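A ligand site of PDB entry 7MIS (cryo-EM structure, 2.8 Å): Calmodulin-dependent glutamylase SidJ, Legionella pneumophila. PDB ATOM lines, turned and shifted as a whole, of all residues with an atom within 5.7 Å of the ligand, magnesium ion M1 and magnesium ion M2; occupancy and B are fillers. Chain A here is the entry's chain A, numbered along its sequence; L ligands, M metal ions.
Two residues have an atom within 4 Å of magnesium ion M2: Asn 439 and Asp 447.
The nearest printed residue that does not touch magnesium ion M2 is Tyr 437 (4.03 Å).
Magnesium ion M2 is bound by an oxygen (O4) of the ligand (1.9 Å), the side-chain amide oxygen (OD1) of Asn 439 (2.0 Å) and an oxygen (O1) of the ligand (2.6 Å).
Magnesium ion M2 has three donor atoms within binding distance.
NZ of Lys 272 is in salt-bridge range of O2 of the ligand (3.4 Å).
The side-chain amino group (NZ) of Lys 275 lies within salt-bridge range of an oxygen (O7) of the ligand (3.5 Å).
A nitrogen (N5) of the ligand lies within hydrogen-bond range of the side-chain hydroxyl of Tyr 437.
N5 of the ligand is in hydrogen-bond range of NH1 of Arg 332 (2.6 Å).
N3 of the ligand sits at hydrogen-bond distance from OH of Tyr 357.
O3 of the ligand lies within salt-bridge range of NH2 of Arg 441.
The guanidinium group of Arg 257 lies within salt-bridge range of an oxygen (O7) of the ligand (3.4 Å).
NE2 of Gln 255 is in hydrogen-bond range of OH of Tyr 357 (3.4 Å).
OE1 of Glu 286 is in salt-bridge range of NZ of Lys 272.
The side-chain amino group of Lys 272 lies within salt-bridge range of the side-chain carboxylate of Asp 447 (3.5 Å).
NH1 of Arg 441 lies within hydrogen-bond range of O of Tyr 354.
The backbone carbonyl oxygen (O) of Asn 439 is in hydrogen-bond range of the backbone NH (N) of Ala 446.
NE of Arg 441 is in hydrogen-bond range of O of Val 438 (3.2 Å).
ND2 of Asn 439 lies within hydrogen-bond range of O of Gln 391 (3.0 Å).
The nearest printed residue that does not touch magnesium ion M1 is Arg 257 (4.4 Å).
Gln 255 touches the ligand.
Gly 256 touches the ligand.
CD1 of Leu 336 touches O11 of the ligand, at 3.5 Å.
The nearest printed residue that does not touch the ligand is Thr 258 (4.4 Å).
Magnesium ion M1 is bound by the side-chain carboxylate of Asp 447, the side-chain carboxylate of Asp 450 and an oxygen (O5) of the ligand.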
ATOM      1  N   GLN A 255      -4.860  -7.351 -23.325  1.00  0.00           N
ATOM      2  CA  GLN A 255      -4.632  -6.258 -22.398  1.00  0.00           C
ATOM      3  C   GLN A 255      -4.149  -6.809 -21.064  1.00  0.00           C
ATOM      4  O   GLN A 255      -4.762  -7.715 -20.503  1.00  0.00           O
ATOM      5  CB  GLN A 255      -5.891  -5.392 -22.212  1.00  0.00           C
ATOM      6  CG  GLN A 255      -6.976  -5.969 -21.347  1.00  0.00           C
ATOM      7  CD  GLN A 255      -8.131  -5.005 -21.179  1.00  0.00           C
ATOM      8  OE1 GLN A 255      -8.660  -4.478 -22.163  1.00  0.00           O
ATOM      9  NE2 GLN A 255      -8.526  -4.761 -19.936  1.00  0.00           N
ATOM     10  N   GLY A 256      -3.029  -6.268 -20.582  1.00  0.00           N
ATOM     11  CA  GLY A 256      -2.430  -6.799 -19.376  1.00  0.00           C
ATOM     12  C   GLY A 256      -2.040  -8.250 -19.581  1.00  0.00           C
ATOM     13  O   GLY A 256      -1.378  -8.603 -20.558  1.00  0.00           O
ATOM     14  N   ARG A 257      -2.472  -9.091 -18.658  1.00  0.00           N
ATOM     15  CA  ARG A 257      -2.277 -10.530 -18.741  1.00  0.00           C
ATOM     16  C   ARG A 257      -3.539 -11.251 -19.207  1.00  0.00           C
ATOM     17  O   ARG A 257      -3.738 -12.428 -18.889  1.00  0.00           O
ATOM     18  CB  ARG A 257      -1.835 -11.081 -17.386  1.00  0.00           C
ATOM     19  CG  ARG A 257      -2.933 -11.087 -16.342  1.00  0.00           C
ATOM     20  CD  ARG A 257      -2.390 -11.296 -14.955  1.00  0.00           C
ATOM     21  NE  ARG A 257      -3.455 -11.585 -14.003  1.00  0.00           N
ATOM     22  CZ  ARG A 257      -3.341 -11.477 -12.690  1.00  0.00           C
ATOM     23  NH1 ARG A 257      -2.216 -11.091 -12.122  1.00  0.00           N
ATOM     24  NH2 ARG A 257      -4.384 -11.776 -11.914  1.00  0.00           N
ATOM     25  N   THR A 258      -4.400 -10.565 -19.963  1.00  0.00           N
ATOM     26  CA  THR A 258      -5.683 -11.110 -20.361  1.00  0.00           C
ATOM     27  C   THR A 258      -5.813 -11.119 -21.884  1.00  0.00           C
ATOM     28  O   THR A 258      -5.472 -10.146 -22.563  1.00  0.00           O
ATOM     29  CB  THR A 258      -6.838 -10.301 -19.757  1.00  0.00           C
ATOM     30  OG1 THR A 258      -6.695 -10.273 -18.330  1.00  0.00           O
ATOM     31  CG2 THR A 258      -8.177 -10.930 -20.101  1.00  0.00           C
ATOM     32  N   LYS A 272      -7.452 -15.199 -18.409  1.00  0.00           N
ATOM     33  CA  LYS A 272      -6.487 -14.512 -17.552  1.00  0.00           C
ATOM     34  C   LYS A 272      -5.359 -15.486 -17.256  1.00  0.00           C
ATOM     35  O   LYS A 272      -5.575 -16.497 -16.579  1.00  0.00           O
ATOM     36  CB  LYS A 272      -7.179 -14.039 -16.273  1.00  0.00           C
ATOM     37  CG  LYS A 272      -6.536 -12.855 -15.598  1.00  0.00           C
ATOM     38  CD  LYS A 272      -7.044 -12.723 -14.180  1.00  0.00           C
ATOM     39  CE  LYS A 272      -7.130 -11.275 -13.751  1.00  0.00           C
ATOM     40  NZ  LYS A 272      -7.628 -11.145 -12.354  1.00  0.00           N
ATOM     41  N   LYS A 275       0.298 -14.708 -13.644  1.00  0.00           N
ATOM     42  CA  LYS A 275       1.398 -13.755 -13.603  1.00  0.00           C
ATOM     43  C   LYS A 275       2.637 -14.407 -13.001  1.00  0.00           C
ATOM     44  O   LYS A 275       2.577 -15.498 -12.422  1.00  0.00           O
ATOM     45  CB  LYS A 275       0.983 -12.517 -12.808  1.00  0.00           C
ATOM     46  CG  LYS A 275       1.802 -11.273 -13.118  1.00  0.00           C
ATOM     47  CD  LYS A 275       1.184 -10.038 -12.497  1.00  0.00           C
ATOM     48  CE  LYS A 275       1.197 -10.100 -10.979  1.00  0.00           C
ATOM     49  NZ  LYS A 275       0.769  -8.826 -10.354  1.00  0.00           N
ATOM     50  N   GLU A 286     -10.209 -15.737  -7.154  1.00  0.00           N
ATOM     51  CA  GLU A 286     -11.017 -14.890  -8.020  1.00  0.00           C
ATOM     52  C   GLU A 286     -12.223 -15.653  -8.563  1.00  0.00           C
ATOM     53  O   GLU A 286     -13.342 -15.130  -8.598  1.00  0.00           O
ATOM     54  CB  GLU A 286     -10.178 -14.331  -9.165  1.00  0.00           C
ATOM     55  CG  GLU A 286     -10.953 -13.429 -10.112  1.00  0.00           C
ATOM     56  CD  GLU A 286     -10.060 -12.518 -10.923  1.00  0.00           C
ATOM     57  OE1 GLU A 286      -8.821 -12.542 -10.709  1.00  0.00           O
ATOM     58  OE2 GLU A 286     -10.584 -11.786 -11.787  1.00  0.00           O
ATOM     59  N   ARG A 332       5.004  -7.306 -24.681  1.00  0.00           N
ATOM     60  CA  ARG A 332       4.638  -6.954 -23.316  1.00  0.00           C
ATOM     61  C   ARG A 332       3.883  -8.099 -22.645  1.00  0.00           C
ATOM     62  O   ARG A 332       4.142  -8.427 -21.482  1.00  0.00           O
ATOM     63  CB  ARG A 332       3.812  -5.671 -23.315  1.00  0.00           C
ATOM     64  CG  ARG A 332       3.422  -5.170 -21.939  1.00  0.00           C
ATOM     65  CD  ARG A 332       2.605  -3.886 -22.025  1.00  0.00           C
ATOM     66  NE  ARG A 332       1.341  -4.081 -22.709  1.00  0.00           N
ATOM     67  CZ  ARG A 332       0.238  -4.547 -22.148  1.00  0.00           C
ATOM     68  NH1 ARG A 332       0.204  -4.868 -20.860  1.00  0.00           N
ATOM     69  NH2 ARG A 332      -0.862  -4.696 -22.874  1.00  0.00           N
ATOM     70  N   LEU A 336       5.027 -10.162 -19.272  1.00  0.00           N
ATOM     71  CA  LEU A 336       4.159 -10.182 -18.099  1.00  0.00           C
ATOM     72  C   LEU A 336       3.928 -11.602 -17.589  1.00  0.00           C
ATOM     73  O   LEU A 336       4.027 -11.855 -16.390  1.00  0.00           O
ATOM     74  CB  LEU A 336       2.822  -9.501 -18.414  1.00  0.00           C
ATOM     75  CG  LEU A 336       2.855  -8.001 -18.709  1.00  0.00           C
ATOM     76  CD1 LEU A 336       1.483  -7.529 -19.144  1.00  0.00           C
ATOM     77  CD2 LEU A 336       3.330  -7.237 -17.485  1.00  0.00           C
ATOM     78  N   TYR A 348     -13.367 -16.581 -18.058  1.00  0.00           N
ATOM     79  CA  TYR A 348     -14.693 -16.089 -17.712  1.00  0.00           C
ATOM     80  C   TYR A 348     -15.286 -15.390 -18.923  1.00  0.00           C
ATOM     81  O   TYR A 348     -14.630 -15.185 -19.936  1.00  0.00           O
ATOM     82  CB  TYR A 348     -14.636 -15.152 -16.498  1.00  0.00           C
ATOM     83  CG  TYR A 348     -13.726 -13.955 -16.634  1.00  0.00           C
ATOM     84  CD1 TYR A 348     -12.359 -14.073 -16.466  1.00  0.00           C
ATOM     85  CD2 TYR A 348     -14.244 -12.700 -16.912  1.00  0.00           C
ATOM     86  CE1 TYR A 348     -11.526 -12.980 -16.580  1.00  0.00           C
ATOM     87  CE2 TYR A 348     -13.424 -11.605 -17.028  1.00  0.00           C
ATOM     88  CZ  TYR A 348     -12.061 -11.747 -16.865  1.00  0.00           C
ATOM     89  OH  TYR A 348     -11.236 -10.664 -16.982  1.00  0.00           O
ATOM     90  N   TYR A 354     -17.273  -4.327 -19.487  1.00  0.00           N
ATOM     91  CA  TYR A 354     -16.487  -4.786 -18.351  1.00  0.00           C
ATOM     92  C   TYR A 354     -14.994  -4.527 -18.539  1.00  0.00           C
ATOM     93  O   TYR A 354     -14.260  -4.468 -17.550  1.00  0.00           O
ATOM     94  CB  TYR A 354     -16.726  -6.288 -18.135  1.00  0.00           C
ATOM     95  CG  TYR A 354     -15.938  -6.882 -16.994  1.00  0.00           C
ATOM     96  CD1 TYR A 354     -16.463  -6.928 -15.717  1.00  0.00           C
ATOM     97  CD2 TYR A 354     -14.674  -7.420 -17.210  1.00  0.00           C
ATOM     98  CE1 TYR A 354     -15.745  -7.481 -14.674  1.00  0.00           C
ATOM     99  CE2 TYR A 354     -13.953  -7.963 -16.171  1.00  0.00           C
ATOM    100  CZ  TYR A 354     -14.496  -8.000 -14.908  1.00  0.00           C
ATOM    101  OH  TYR A 354     -13.781  -8.546 -13.877  1.00  0.00           O
ATOM    102  N   TYR A 357     -12.258   0.975 -18.841  1.00  0.00           N
ATOM    103  CA  TYR A 357     -12.071   1.584 -17.538  1.00  0.00           C
ATOM    104  C   TYR A 357     -12.987   2.793 -17.364  1.00  0.00           C
ATOM    105  O   TYR A 357     -13.367   3.456 -18.333  1.00  0.00           O
ATOM    106  CB  TYR A 357     -10.612   1.980 -17.345  1.00  0.00           C
ATOM    107  CG  TYR A 357      -9.680   0.805 -17.487  1.00  0.00           C
ATOM    108  CD1 TYR A 357      -9.494  -0.099 -16.444  1.00  0.00           C
ATOM    109  CD2 TYR A 357      -8.993   0.573 -18.674  1.00  0.00           C
ATOM    110  CE1 TYR A 357      -8.654  -1.173 -16.573  1.00  0.00           C
ATOM    111  CE2 TYR A 357      -8.152  -0.501 -18.803  1.00  0.00           C
ATOM    112  CZ  TYR A 357      -7.983  -1.374 -17.753  1.00  0.00           C
ATOM    113  OH  TYR A 357      -7.143  -2.447 -17.883  1.00  0.00           O
ATOM    114  N   GLN A 391      -7.271  -2.668  -3.069  1.00  0.00           N
ATOM    115  CA  GLN A 391      -6.401  -2.602  -4.242  1.00  0.00           C
ATOM    116  C   GLN A 391      -7.171  -2.147  -5.470  1.00  0.00           C
ATOM    117  O   GLN A 391      -6.912  -2.591  -6.591  1.00  0.00           O
ATOM    118  CB  GLN A 391      -5.739  -3.950  -4.501  1.00  0.00           C
ATOM    119  CG  GLN A 391      -4.656  -4.300  -3.508  1.00  0.00           C
ATOM    120  CD  GLN A 391      -3.972  -5.613  -3.846  1.00  0.00           C
ATOM    121  OE1 GLN A 391      -4.404  -6.678  -3.413  1.00  0.00           O
ATOM    122  NE2 GLN A 391      -2.912  -5.532  -4.637  1.00  0.00           N
ATOM    123  N   TYR A 437      -5.225   1.652 -14.688  1.00  0.00           N
ATOM    124  CA  TYR A 437      -5.773   0.301 -14.700  1.00  0.00           C
ATOM    125  C   TYR A 437      -6.671   0.087 -13.495  1.00  0.00           C
ATOM    126  O   TYR A 437      -6.619  -0.947 -12.825  1.00  0.00           O
ATOM    127  CB  TYR A 437      -4.653  -0.746 -14.726  1.00  0.00           C
ATOM    128  CG  TYR A 437      -3.626  -0.508 -15.805  1.00  0.00           C
ATOM    129  CD1 TYR A 437      -4.015  -0.308 -17.121  1.00  0.00           C
ATOM    130  CD2 TYR A 437      -2.277  -0.490 -15.509  1.00  0.00           C
ATOM    131  CE1 TYR A 437      -3.089  -0.090 -18.111  1.00  0.00           C
ATOM    132  CE2 TYR A 437      -1.338  -0.274 -16.497  1.00  0.00           C
ATOM    133  CZ  TYR A 437      -1.744  -0.074 -17.798  1.00  0.00           C
ATOM    134  OH  TYR A 437      -0.811   0.146 -18.781  1.00  0.00           O
ATOM    135  N   VAL A 438      -7.507   1.083 -13.191  1.00  0.00           N
ATOM    136  CA  VAL A 438      -8.356   1.009 -12.021  1.00  0.00           C
ATOM    137  C   VAL A 438      -9.337  -0.159 -12.151  1.00  0.00           C
ATOM    138  O   VAL A 438      -9.774  -0.518 -13.251  1.00  0.00           O
ATOM    139  CB  VAL A 438      -9.105   2.338 -11.831  1.00  0.00           C
ATOM    140  CG1 VAL A 438     -10.101   2.562 -12.960  1.00  0.00           C
ATOM    141  CG2 VAL A 438      -9.800   2.384 -10.487  1.00  0.00           C
ATOM    142  N   ASN A 439      -9.665  -0.766 -11.012  1.00  0.00           N
ATOM    143  CA  ASN A 439     -10.572  -1.902 -10.986  1.00  0.00           C
ATOM    144  C   ASN A 439     -12.034  -1.497 -10.996  1.00  0.00           C
ATOM    145  O   ASN A 439     -12.893  -2.333 -10.697  1.00  0.00           O
ATOM    146  CB  ASN A 439     -10.273  -2.770  -9.753  1.00  0.00           C
ATOM    147  CG  ASN A 439      -9.061  -3.645  -9.938  1.00  0.00           C
ATOM    148  OD1 ASN A 439      -8.708  -4.018 -11.047  1.00  0.00           O
ATOM    149  ND2 ASN A 439      -8.400  -3.989  -8.830  1.00  0.00           N
ATOM    150  N   ARG A 441     -14.951  -0.239 -13.602  1.00  0.00           N
ATOM    151  CA  ARG A 441     -15.175  -0.319 -15.042  1.00  0.00           C
ATOM    152  C   ARG A 441     -16.514   0.319 -15.398  1.00  0.00           C
ATOM    153  O   ARG A 441     -17.306   0.692 -14.530  1.00  0.00           O
ATOM    154  CB  ARG A 441     -15.152  -1.764 -15.524  1.00  0.00           C
ATOM    155  CG  ARG A 441     -13.916  -2.526 -15.105  1.00  0.00           C
ATOM    156  CD  ARG A 441     -12.651  -1.981 -15.741  1.00  0.00           C
ATOM    157  NE  ARG A 441     -11.463  -2.512 -15.085  1.00  0.00           N
ATOM    158  CZ  ARG A 441     -11.027  -3.753 -15.233  1.00  0.00           C
ATOM    159  NH1 ARG A 441     -11.635  -4.616 -16.028  1.00  0.00           N
ATOM    160  NH2 ARG A 441      -9.942  -4.134 -14.566  1.00  0.00           N
ATOM    161  N   ALA A 446     -14.501  -5.011 -11.146  1.00  0.00           N
ATOM    162  CA  ALA A 446     -13.823  -5.927 -12.067  1.00  0.00           C
ATOM    163  C   ALA A 446     -12.966  -6.972 -11.367  1.00  0.00           C
ATOM    164  O   ALA A 446     -13.207  -8.169 -11.567  1.00  0.00           O
ATOM    165  CB  ALA A 446     -12.971  -5.118 -13.044  1.00  0.00           C
ATOM    166  N   ASP A 447     -11.983  -6.570 -10.564  1.00  0.00           N
ATOM    167  CA  ASP A 447     -10.984  -7.514 -10.047  1.00  0.00           C
ATOM    168  C   ASP A 447     -11.445  -7.995  -8.681  1.00  0.00           C
ATOM    169  O   ASP A 447     -10.944  -7.587  -7.632  1.00  0.00           O
ATOM    170  CB  ASP A 447      -9.617  -6.864  -9.998  1.00  0.00           C
ATOM    171  CG  ASP A 447      -8.476  -7.869 -10.091  1.00  0.00           C
ATOM    172  OD1 ASP A 447      -8.711  -9.057  -9.794  1.00  0.00           O
ATOM    173  OD2 ASP A 447      -7.361  -7.463 -10.462  1.00  0.00           O
ATOM    174  N   ASP A 450      -9.144  -9.709  -5.606  1.00  0.00           N
ATOM    175  CA  ASP A 450      -8.211  -8.934  -4.797  1.00  0.00           C
ATOM    176  C   ASP A 450      -8.956  -8.229  -3.663  1.00  0.00           C
ATOM    177  O   ASP A 450      -9.052  -7.010  -3.596  1.00  0.00           O
ATOM    178  CB  ASP A 450      -7.457  -7.933  -5.672  1.00  0.00           C
ATOM    179  CG  ASP A 450      -6.623  -8.610  -6.742  1.00  0.00           C
ATOM    180  OD1 ASP A 450      -5.992  -9.644  -6.439  1.00  0.00           O
ATOM    181  OD2 ASP A 450      -6.584  -8.093  -7.882  1.00  0.00           O
HETATM  182  P1  LIG L   1      -8.017  -7.127 -14.481  1.00  0.00           P
HETATM  183  O1  LIG L   1      -8.425  -5.955 -13.676  1.00  0.00           O
HETATM  184  O2  LIG L   1      -8.747  -8.403 -14.092  1.00  0.00           O
HETATM  185  O3  LIG L   1      -8.169  -6.904 -15.988  1.00  0.00           O
HETATM  186  P2  LIG L   1      -5.519  -7.363 -13.004  1.00  0.00           P
HETATM  187  O4  LIG L   1      -5.659  -6.064 -12.322  1.00  0.00           O
HETATM  188  O5  LIG L   1      -5.745  -8.599 -12.159  1.00  0.00           O
HETATM  189  O6  LIG L   1      -6.476  -7.470 -14.273  1.00  0.00           O
HETATM  190  P3  LIG L   1      -2.657  -6.903 -13.289  1.00  0.00           P
HETATM  191  O7  LIG L   1      -2.036  -7.661 -12.182  1.00  0.00           O
HETATM  192  O8  LIG L   1      -2.878  -5.419 -13.008  1.00  0.00           O
HETATM  193  O9  LIG L   1      -4.081  -7.515 -13.672  1.00  0.00           O
HETATM  194  O10 LIG L   1      -1.778  -6.981 -14.634  1.00  0.00           O
HETATM  195  C1  LIG L   1      -0.335  -7.123 -14.591  1.00  0.00           C
HETATM  196  C2  LIG L   1       0.294  -5.953 -15.308  1.00  0.00           C
HETATM  197  O11 LIG L   1      -0.237  -5.863 -16.650  1.00  0.00           O
HETATM  198  C3  LIG L   1       0.038  -4.594 -14.689  1.00  0.00           C
HETATM  199  O12 LIG L   1       0.959  -4.320 -13.643  1.00  0.00           O
HETATM  200  C4  LIG L   1       0.231  -3.656 -15.887  1.00  0.00           C
HETATM  201  O13 LIG L   1       1.604  -3.348 -16.093  1.00  0.00           O
HETATM  202  C5  LIG L   1      -0.294  -4.502 -17.049  1.00  0.00           C
HETATM  203  N1  LIG L   1      -1.674  -4.209 -17.434  1.00  0.00           N
HETATM  204  C6  LIG L   1      -2.809  -4.478 -16.720  1.00  0.00           C
HETATM  205  N2  LIG L   1      -3.920  -4.126 -17.319  1.00  0.00           N
HETATM  206  C7  LIG L   1      -3.482  -3.566 -18.513  1.00  0.00           C
HETATM  207  C8  LIG L   1      -4.166  -3.006 -19.613  1.00  0.00           C
HETATM  208  N3  LIG L   1      -5.490  -2.911 -19.638  1.00  0.00           N
HETATM  209  N4  LIG L   1      -3.434  -2.560 -20.654  1.00  0.00           N
HETATM  210  C9  LIG L   1      -2.103  -2.662 -20.593  1.00  0.00           C
HETATM  211  N5  LIG L   1      -1.344  -3.174 -19.607  1.00  0.00           N
HETATM  212  C10 LIG L   1      -2.106  -3.613 -18.595  1.00  0.00           C
HETATM  213 MG    MG M   1      -5.521  -8.067  -9.805  1.00  0.00          MG
HETATM  214 MG    MG M   2      -7.027  -4.822 -11.803  1.00  0.00          MG
